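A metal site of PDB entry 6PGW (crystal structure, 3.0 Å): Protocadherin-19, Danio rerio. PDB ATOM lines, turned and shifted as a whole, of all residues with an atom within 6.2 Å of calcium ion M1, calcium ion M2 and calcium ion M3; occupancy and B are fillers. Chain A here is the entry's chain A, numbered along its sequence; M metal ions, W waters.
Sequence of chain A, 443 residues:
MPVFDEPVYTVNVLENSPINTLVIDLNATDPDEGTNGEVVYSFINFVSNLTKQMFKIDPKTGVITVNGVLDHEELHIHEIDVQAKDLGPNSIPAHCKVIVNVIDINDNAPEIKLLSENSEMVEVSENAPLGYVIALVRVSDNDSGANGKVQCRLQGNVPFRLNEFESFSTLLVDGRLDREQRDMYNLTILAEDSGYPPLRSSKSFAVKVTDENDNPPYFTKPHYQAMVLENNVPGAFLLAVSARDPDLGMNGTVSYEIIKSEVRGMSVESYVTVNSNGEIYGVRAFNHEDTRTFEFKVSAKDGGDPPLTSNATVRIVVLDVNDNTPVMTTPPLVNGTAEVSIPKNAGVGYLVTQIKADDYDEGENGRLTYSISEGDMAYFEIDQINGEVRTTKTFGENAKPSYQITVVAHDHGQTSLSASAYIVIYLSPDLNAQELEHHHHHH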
ATOM      1  N   GLU A 230      23.131 -20.604 -20.221  1.00  0.00           N
ATOM      2  CA  GLU A 230      23.776 -21.396 -21.242  1.00  0.00           C
ATOM      3  C   GLU A 230      25.303 -21.169 -21.183  1.00  0.00           C
ATOM      4  O   GLU A 230      25.767 -20.143 -20.677  1.00  0.00           O
ATOM      5  CB  GLU A 230      23.141 -20.993 -22.590  1.00  0.00           C
ATOM      6  CG  GLU A 230      23.961 -21.193 -23.809  1.00  0.00           C
ATOM      7  CD  GLU A 230      23.163 -20.985 -25.073  1.00  0.00           C
ATOM      8  OE1 GLU A 230      22.377 -20.001 -25.200  1.00  0.00           O
ATOM      9  OE2 GLU A 230      23.345 -21.794 -25.957  1.00  0.00           O
ATOM     10  N   ASN A 231      26.071 -22.169 -21.623  1.00  0.00           N
ATOM     11  CA  ASN A 231      27.555 -22.142 -21.556  1.00  0.00           C
ATOM     12  C   ASN A 231      28.127 -22.039 -20.112  1.00  0.00           C
ATOM     13  O   ASN A 231      29.167 -21.410 -19.893  1.00  0.00           O
ATOM     14  CB  ASN A 231      28.126 -20.999 -22.420  1.00  0.00           C
ATOM     15  CG  ASN A 231      27.595 -21.018 -23.832  1.00  0.00           C
ATOM     16  OD1 ASN A 231      27.278 -22.066 -24.357  1.00  0.00           O
ATOM     17  ND2 ASN A 231      27.494 -19.847 -24.442  1.00  0.00           N
ATOM     18  N   PHE A 286      25.988 -26.697 -20.706  1.00  0.00           N
ATOM     19  CA  PHE A 286      24.659 -26.690 -21.348  1.00  0.00           C
ATOM     20  C   PHE A 286      24.560 -25.685 -22.528  1.00  0.00           C
ATOM     21  O   PHE A 286      25.270 -24.676 -22.580  1.00  0.00           O
ATOM     22  CB  PHE A 286      23.562 -26.386 -20.314  1.00  0.00           C
ATOM     23  CG  PHE A 286      23.514 -27.354 -19.150  1.00  0.00           C
ATOM     24  CD1 PHE A 286      23.819 -28.698 -19.294  1.00  0.00           C
ATOM     25  CD2 PHE A 286      23.085 -26.914 -17.900  1.00  0.00           C
ATOM     26  CE1 PHE A 286      23.749 -29.561 -18.216  1.00  0.00           C
ATOM     27  CE2 PHE A 286      23.022 -27.783 -16.821  1.00  0.00           C
ATOM     28  CZ  PHE A 286      23.354 -29.100 -16.982  1.00  0.00           C
ATOM     29  N   ASN A 287      23.646 -25.968 -23.454  1.00  0.00           N
ATOM     30  CA  ASN A 287      23.480 -25.216 -24.697  1.00  0.00           C
ATOM     31  C   ASN A 287      22.010 -25.170 -25.104  1.00  0.00           C
ATOM     32  O   ASN A 287      21.482 -26.118 -25.644  1.00  0.00           O
ATOM     33  CB  ASN A 287      24.280 -25.865 -25.807  1.00  0.00           C
ATOM     34  CG  ASN A 287      24.066 -25.177 -27.152  1.00  0.00           C
ATOM     35  OD1 ASN A 287      23.512 -24.070 -27.235  1.00  0.00           O
ATOM     36  ND2 ASN A 287      24.515 -25.841 -28.200  1.00  0.00           N
ATOM     37  N   HIS A 288      21.388 -24.021 -24.854  1.00  0.00           N
ATOM     38  CA  HIS A 288      19.990 -23.729 -25.184  1.00  0.00           C
ATOM     39  C   HIS A 288      19.548 -24.114 -26.607  1.00  0.00           C
ATOM     40  O   HIS A 288      18.375 -24.322 -26.885  1.00  0.00           O
ATOM     41  CB  HIS A 288      19.784 -22.242 -24.983  1.00  0.00           C
ATOM     42  CG  HIS A 288      18.412 -21.768 -25.302  1.00  0.00           C
ATOM     43  ND1 HIS A 288      17.496 -21.464 -24.317  1.00  0.00           N
ATOM     44  CD2 HIS A 288      17.806 -21.493 -26.481  1.00  0.00           C
ATOM     45  CE1 HIS A 288      16.370 -21.051 -24.878  1.00  0.00           C
ATOM     46  NE2 HIS A 288      16.530 -21.067 -26.191  1.00  0.00           N
ATOM     47  N   GLU A 289      20.497 -24.184 -27.512  1.00  0.00           N
ATOM     48  CA  GLU A 289      20.207 -24.572 -28.852  1.00  0.00           C
ATOM     49  C   GLU A 289      20.138 -26.140 -28.982  1.00  0.00           C
ATOM     50  O   GLU A 289      19.722 -26.686 -30.012  1.00  0.00           O
ATOM     51  CB  GLU A 289      21.267 -23.944 -29.750  1.00  0.00           C
ATOM     52  CG  GLU A 289      21.072 -22.428 -29.966  1.00  0.00           C
ATOM     53  CD  GLU A 289      21.329 -21.560 -28.735  1.00  0.00           C
ATOM     54  OE1 GLU A 289      20.545 -20.634 -28.411  1.00  0.00           O
ATOM     55  OE2 GLU A 289      22.330 -21.787 -28.069  1.00  0.00           O
ATOM     56  N   LEU A 319      18.539 -21.055 -19.972  1.00  0.00           N
ATOM     57  CA  LEU A 319      18.266 -19.719 -20.439  1.00  0.00           C
ATOM     58  C   LEU A 319      19.144 -19.331 -21.636  1.00  0.00           C
ATOM     59  O   LEU A 319      20.256 -19.811 -21.780  1.00  0.00           O
ATOM     60  CB  LEU A 319      18.510 -18.749 -19.321  1.00  0.00           C
ATOM     61  CG  LEU A 319      17.752 -19.013 -18.018  1.00  0.00           C
ATOM     62  CD1 LEU A 319      18.299 -18.106 -16.931  1.00  0.00           C
ATOM     63  CD2 LEU A 319      16.254 -18.811 -18.179  1.00  0.00           C
ATOM     64  N   ASP A 320      18.628 -18.453 -22.476  1.00  0.00           N
ATOM     65  CA  ASP A 320      19.272 -18.104 -23.739  1.00  0.00           C
ATOM     66  C   ASP A 320      20.287 -17.015 -23.495  1.00  0.00           C
ATOM     67  O   ASP A 320      19.985 -16.000 -22.839  1.00  0.00           O
ATOM     68  CB  ASP A 320      18.214 -17.634 -24.738  1.00  0.00           C
ATOM     69  CG  ASP A 320      18.788 -17.313 -26.137  1.00  0.00           C
ATOM     70  OD1 ASP A 320      19.723 -18.028 -26.637  1.00  0.00           O
ATOM     71  OD2 ASP A 320      18.268 -16.341 -26.734  1.00  0.00           O
ATOM     72  N   VAL A 321      21.477 -17.227 -24.023  1.00  0.00           N
ATOM     73  CA  VAL A 321      22.442 -16.159 -24.198  1.00  0.00           C
ATOM     74  C   VAL A 321      22.822 -16.034 -25.673  1.00  0.00           C
ATOM     75  O   VAL A 321      22.730 -17.022 -26.445  1.00  0.00           O
ATOM     76  CB  VAL A 321      23.688 -16.337 -23.301  1.00  0.00           C
ATOM     77  CG1 VAL A 321      23.273 -16.611 -21.863  1.00  0.00           C
ATOM     78  CG2 VAL A 321      24.585 -17.461 -23.819  1.00  0.00           C
ATOM     79  N   ASN A 322      23.212 -14.807 -26.038  1.00  0.00           N
ATOM     80  CA  ASN A 322      23.455 -14.424 -27.416  1.00  0.00           C
ATOM     81  C   ASN A 322      24.837 -14.927 -27.811  1.00  0.00           C
ATOM     82  O   ASN A 322      25.770 -14.147 -27.986  1.00  0.00           O
ATOM     83  CB  ASN A 322      23.353 -12.885 -27.594  1.00  0.00           C
ATOM     84  CG  ASN A 322      23.360 -12.456 -29.058  1.00  0.00           C
ATOM     85  OD1 ASN A 322      23.093 -13.279 -29.965  1.00  0.00           O
ATOM     86  ND2 ASN A 322      23.669 -11.169 -29.311  1.00  0.00           N
ATOM     87  N   ASP A 323      24.937 -16.236 -27.976  1.00  0.00           N
ATOM     88  CA  ASP A 323      26.202 -16.931 -28.148  1.00  0.00           C
ATOM     89  C   ASP A 323      26.285 -17.510 -29.525  1.00  0.00           C
ATOM     90  O   ASP A 323      27.056 -18.421 -29.799  1.00  0.00           O
ATOM     91  CB  ASP A 323      26.330 -18.034 -27.096  1.00  0.00           C
ATOM     92  CG  ASP A 323      25.277 -19.163 -27.232  1.00  0.00           C
ATOM     93  OD1 ASP A 323      24.097 -18.935 -27.686  1.00  0.00           O
ATOM     94  OD2 ASP A 323      25.632 -20.288 -26.840  1.00  0.00           O
ATOM     95  N   ASN A 324      25.455 -16.966 -30.399  1.00  0.00           N
ATOM     96  CA  ASN A 324      25.487 -17.281 -31.792  1.00  0.00           C
ATOM     97  C   ASN A 324      25.412 -15.983 -32.537  1.00  0.00           C
ATOM     98  O   ASN A 324      24.347 -15.227 -32.471  1.00  0.00           O
ATOM     99  CB  ASN A 324      24.304 -18.126 -32.205  1.00  0.00           C
ATOM    100  CG  ASN A 324      24.426 -19.546 -31.787  1.00  0.00           C
ATOM    101  OD1 ASN A 324      25.234 -20.290 -32.314  1.00  0.00           O
ATOM    102  ND2 ASN A 324      23.564 -19.943 -30.860  1.00  0.00           N
ATOM    103  N   THR A 325      26.546 -15.681 -33.180  1.00  0.00           N
ATOM    104  CA  THR A 325      26.653 -14.696 -34.259  1.00  0.00           C
ATOM    105  C   THR A 325      25.845 -15.198 -35.452  1.00  0.00           C
ATOM    106  O   THR A 325      25.914 -16.367 -35.792  1.00  0.00           O
ATOM    107  CB  THR A 325      28.121 -14.540 -34.738  1.00  0.00           C
ATOM    108  OG1 THR A 325      28.705 -15.843 -34.856  1.00  0.00           O
ATOM    109  CG2 THR A 325      28.962 -13.718 -33.792  1.00  0.00           C
ATOM    110  N   PRO A 326      25.117 -14.279 -36.121  1.00  0.00           N
ATOM    111  CA  PRO A 326      24.257 -14.606 -37.281  1.00  0.00           C
ATOM    112  C   PRO A 326      25.016 -15.182 -38.474  1.00  0.00           C
ATOM    113  O   PRO A 326      26.218 -14.999 -38.566  1.00  0.00           O
ATOM    114  CB  PRO A 326      23.679 -13.252 -37.678  1.00  0.00           C
ATOM    115  CG  PRO A 326      23.788 -12.405 -36.469  1.00  0.00           C
ATOM    116  CD  PRO A 326      24.969 -12.877 -35.702  1.00  0.00           C
ATOM    117  N   ASP A 359      19.942 -16.971 -37.429  1.00  0.00           N
ATOM    118  CA  ASP A 359      20.593 -16.830 -36.075  1.00  0.00           C
ATOM    119  C   ASP A 359      19.832 -17.810 -35.184  1.00  0.00           C
ATOM    120  O   ASP A 359      18.605 -17.875 -35.232  1.00  0.00           O
ATOM    121  CB  ASP A 359      20.456 -15.389 -35.531  1.00  0.00           C
ATOM    122  CG  ASP A 359      21.254 -15.126 -34.224  1.00  0.00           C
ATOM    123  OD1 ASP A 359      21.123 -15.851 -33.252  1.00  0.00           O
ATOM    124  OD2 ASP A 359      21.923 -14.118 -34.152  1.00  0.00           O
ATOM    125  N   TYR A 360      20.543 -18.603 -34.398  1.00  0.00           N
ATOM    126  CA  TYR A 360      19.899 -19.691 -33.664  1.00  0.00           C
ATOM    127  C   TYR A 360      19.330 -19.322 -32.360  1.00  0.00           C
ATOM    128  O   TYR A 360      18.358 -19.943 -31.896  1.00  0.00           O
ATOM    129  CB  TYR A 360      20.866 -20.849 -33.503  1.00  0.00           C
ATOM    130  CG  TYR A 360      21.426 -21.284 -34.842  1.00  0.00           C
ATOM    131  CD1 TYR A 360      20.584 -21.478 -35.946  1.00  0.00           C
ATOM    132  CD2 TYR A 360      22.786 -21.411 -35.028  1.00  0.00           C
ATOM    133  CE1 TYR A 360      21.088 -21.857 -37.171  1.00  0.00           C
ATOM    134  CE2 TYR A 360      23.305 -21.774 -36.257  1.00  0.00           C
ATOM    135  CZ  TYR A 360      22.442 -22.005 -37.316  1.00  0.00           C
ATOM    136  OH  TYR A 360      22.952 -22.363 -38.517  1.00  0.00           O
ATOM    137  N   ASP A 361      19.841 -18.277 -31.763  1.00  0.00           N
ATOM    138  CA  ASP A 361      19.360 -17.889 -30.493  1.00  0.00           C
ATOM    139  C   ASP A 361      17.861 -17.589 -30.581  1.00  0.00           C
ATOM    140  O   ASP A 361      17.306 -17.476 -31.685  1.00  0.00           O
ATOM    141  CB  ASP A 361      20.119 -16.706 -29.970  1.00  0.00           C
ATOM    142  CG  ASP A 361      21.617 -16.966 -29.878  1.00  0.00           C
ATOM    143  OD1 ASP A 361      22.018 -18.073 -29.381  1.00  0.00           O
ATOM    144  OD2 ASP A 361      22.385 -16.025 -30.281  1.00  0.00           O
ATOM    145  N   GLU A 362      17.205 -17.535 -29.448  1.00  0.00           N
ATOM    146  CA  GLU A 362      15.774 -17.251 -29.425  1.00  0.00           C
ATOM    147  C   GLU A 362      15.570 -15.835 -28.931  1.00  0.00           C
ATOM    148  O   GLU A 362      16.400 -15.293 -28.217  1.00  0.00           O
ATOM    149  CB  GLU A 362      15.057 -18.243 -28.539  1.00  0.00           C
ATOM    150  CG  GLU A 362      13.574 -17.928 -28.275  1.00  0.00           C
ATOM    151  CD  GLU A 362      13.207 -17.996 -26.801  1.00  0.00           C
ATOM    152  OE1 GLU A 362      12.030 -17.684 -26.464  1.00  0.00           O
ATOM    153  OE2 GLU A 362      14.069 -18.393 -25.976  1.00  0.00           O
ATOM    154  N   GLU A 364      15.088 -11.775 -28.753  1.00  0.00           N
ATOM    155  CA  GLU A 364      15.824 -10.623 -29.217  1.00  0.00           C
ATOM    156  C   GLU A 364      17.180 -11.052 -29.715  1.00  0.00           C
ATOM    157  O   GLU A 364      17.663 -10.568 -30.722  1.00  0.00           O
ATOM    158  CB  GLU A 364      15.977  -9.603 -28.103  1.00  0.00           C
ATOM    159  CG  GLU A 364      14.679  -8.986 -27.627  1.00  0.00           C
ATOM    160  CD  GLU A 364      14.157  -7.914 -28.572  1.00  0.00           C
ATOM    161  OE1 GLU A 364      14.675  -6.773 -28.528  1.00  0.00           O
ATOM    162  OE2 GLU A 364      13.229  -8.227 -29.359  1.00  0.00           O
ATOM    163  N   ASN A 365      17.748 -12.018 -29.021  1.00  0.00           N
ATOM    164  CA  ASN A 365      19.010 -12.573 -29.359  1.00  0.00           C
ATOM    165  C   ASN A 365      19.013 -13.133 -30.726  1.00  0.00           C
ATOM    166  O   ASN A 365      20.091 -13.287 -31.364  1.00  0.00           O
ATOM    167  CB  ASN A 365      19.343 -13.695 -28.434  1.00  0.00           C
ATOM    168  CG  ASN A 365      19.612 -13.229 -27.025  1.00  0.00           C
ATOM    169  OD1 ASN A 365      20.594 -13.617 -26.424  1.00  0.00           O
ATOM    170  ND2 ASN A 365      18.736 -12.397 -26.495  1.00  0.00           N
ATOM    171  N   GLY A 366      17.847 -13.561 -31.165  1.00  0.00           N
ATOM    172  CA  GLY A 366      17.720 -14.168 -32.447  1.00  0.00           C
ATOM    173  C   GLY A 366      17.135 -13.330 -33.532  1.00  0.00           C
ATOM    174  O   GLY A 366      16.949 -13.827 -34.652  1.00  0.00           O
ATOM    175  N   ARG A 367      16.822 -12.066 -33.224  1.00  0.00           N
ATOM    176  CA  ARG A 367      16.109 -11.202 -34.188  1.00  0.00           C
ATOM    177  C   ARG A 367      17.090 -10.484 -35.106  1.00  0.00           C
ATOM    178  O   ARG A 367      18.130  -9.956 -34.640  1.00  0.00           O
ATOM    179  CB  ARG A 367      15.252 -10.181 -33.470  1.00  0.00           C
ATOM    180  CG  ARG A 367      13.973  -9.795 -34.223  1.00  0.00           C
ATOM    181  CD  ARG A 367      13.209  -8.708 -33.491  1.00  0.00           C
ATOM    182  NE  ARG A 367      13.780  -7.369 -33.689  1.00  0.00           N
ATOM    183  CZ  ARG A 367      14.186  -6.562 -32.723  1.00  0.00           C
ATOM    184  NH1 ARG A 367      14.638  -5.358 -33.021  1.00  0.00           N
ATOM    185  NH2 ARG A 367      14.126  -6.930 -31.442  1.00  0.00           N
ATOM    186  N   ASP A 411      22.037  -8.645 -34.989  1.00  0.00           N
ATOM    187  CA  ASP A 411      20.931  -9.120 -34.138  1.00  0.00           C
ATOM    188  C   ASP A 411      20.642  -8.165 -32.959  1.00  0.00           C
ATOM    189  O   ASP A 411      21.164  -7.034 -32.937  1.00  0.00           O
ATOM    190  CB  ASP A 411      21.142 -10.592 -33.689  1.00  0.00           C
ATOM    191  CG  ASP A 411      22.254 -10.765 -32.631  1.00  0.00           C
ATOM    192  OD1 ASP A 411      22.876  -9.748 -32.219  1.00  0.00           O
ATOM    193  OD2 ASP A 411      22.504 -11.968 -32.226  1.00  0.00           O
ATOM    194  N   LEU A 417      25.459  -9.333 -31.794  1.00  0.00           N
ATOM    195  CA  LEU A 417      26.385  -9.955 -32.735  1.00  0.00           C
ATOM    196  C   LEU A 417      25.949  -9.633 -34.174  1.00  0.00           C
ATOM    197  O   LEU A 417      24.874  -9.043 -34.366  1.00  0.00           O
ATOM    198  CB  LEU A 417      26.519 -11.475 -32.496  1.00  0.00           C
ATOM    199  CG  LEU A 417      27.509 -11.957 -31.390  1.00  0.00           C
ATOM    200  CD1 LEU A 417      28.864 -11.248 -31.466  1.00  0.00           C
ATOM    201  CD2 LEU A 417      26.922 -11.763 -30.003  1.00  0.00           C
HETATM  202 CA    CA M   1      24.600 -22.089 -27.846  1.00  0.00          CA
HETATM  203 CA    CA M   2      21.764 -19.014 -27.242  1.00  0.00          CA
HETATM  204 CA    CA M   3      22.233 -14.301 -31.856  1.00  0.00          CA
HETATM  205  O   HOH W   1      26.016 -23.025 -26.290  1.00  0.00           O
HETATM  206  O   HOH W   2      25.171 -22.122 -30.089  1.00  0.00           O
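The nearest printed residue that does not touch calcium ion M3 is Gly 366 (4.5 Å).
Calcium ion M3 is bound by the side-chain amide oxygen (OD1) of Asn 322 (2.3 Å), the side-chain carboxylate (OD2) of Asp 359 (2.3 Å), the side-chain carboxylate (OD2) of Asp 361 (2.3 Å), the side-chain carboxylate (OD1) of Asp 359 (2.4 Å), the side-chain carboxylate (OD2) of Asp 411 (2.4 Å), the backbone carbonyl oxygen (O) of Asn 324 (2.4 Å) and the backbone carbonyl oxygen (O) of Asn 365 (2.4 Å).
Calcium ion M3 has seven donor atoms within binding distance.
Calcium ion M1 is bound by OE2 of Glu 230, OE2 of Glu 289, water W1, OD2 of Asp 323, water W2 and OD1 of Asn 287.
Within 4 Å of calcium ion M2: Glu 230, Glu 289, Asp 320, Val 321, Asp 323 and Asp 361.
OE2 of Glu 230 sits close to N of His 288.
The backbone NH (N) of Glu 230 lies close to the backbone carbonyl oxygen (O) of Leu 319 (3.4 Å).
OD1 of Asp 323 sits close to ND2 of Asn 324 (3.4 Å).
The side-chain carboxylate (OD2) of Asp 323 sits close to the side-chain amide nitrogen (ND2) of Asn 231 (3.1 Å).
OD2 of Asp 320 is in hydrogen-bond range of N of Glu 362.
OD1 of Asp 411 is in hydrogen-bond range of N of Leu 417, at 2.7 Å.
Calcium ion M2 is bound by the side-chain carboxylate (OE1) of Glu 289 (2.3 Å), the side-chain carboxylate (OD1) of Asp 320 (2.3 Å), the side-chain carboxylate (OE1) of Glu 230 (2.3 Å), the side-chain carboxylate (OD1) of Asp 361 (2.4 Å), the backbone carbonyl oxygen (O) of Val 321 (2.4 Å) and the side-chain carboxylate (OD1) of Asp 323 (2.4 Å).
Slightly farther from calcium ion M2 lies OE2 of Glu 289 (2.9 Å).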
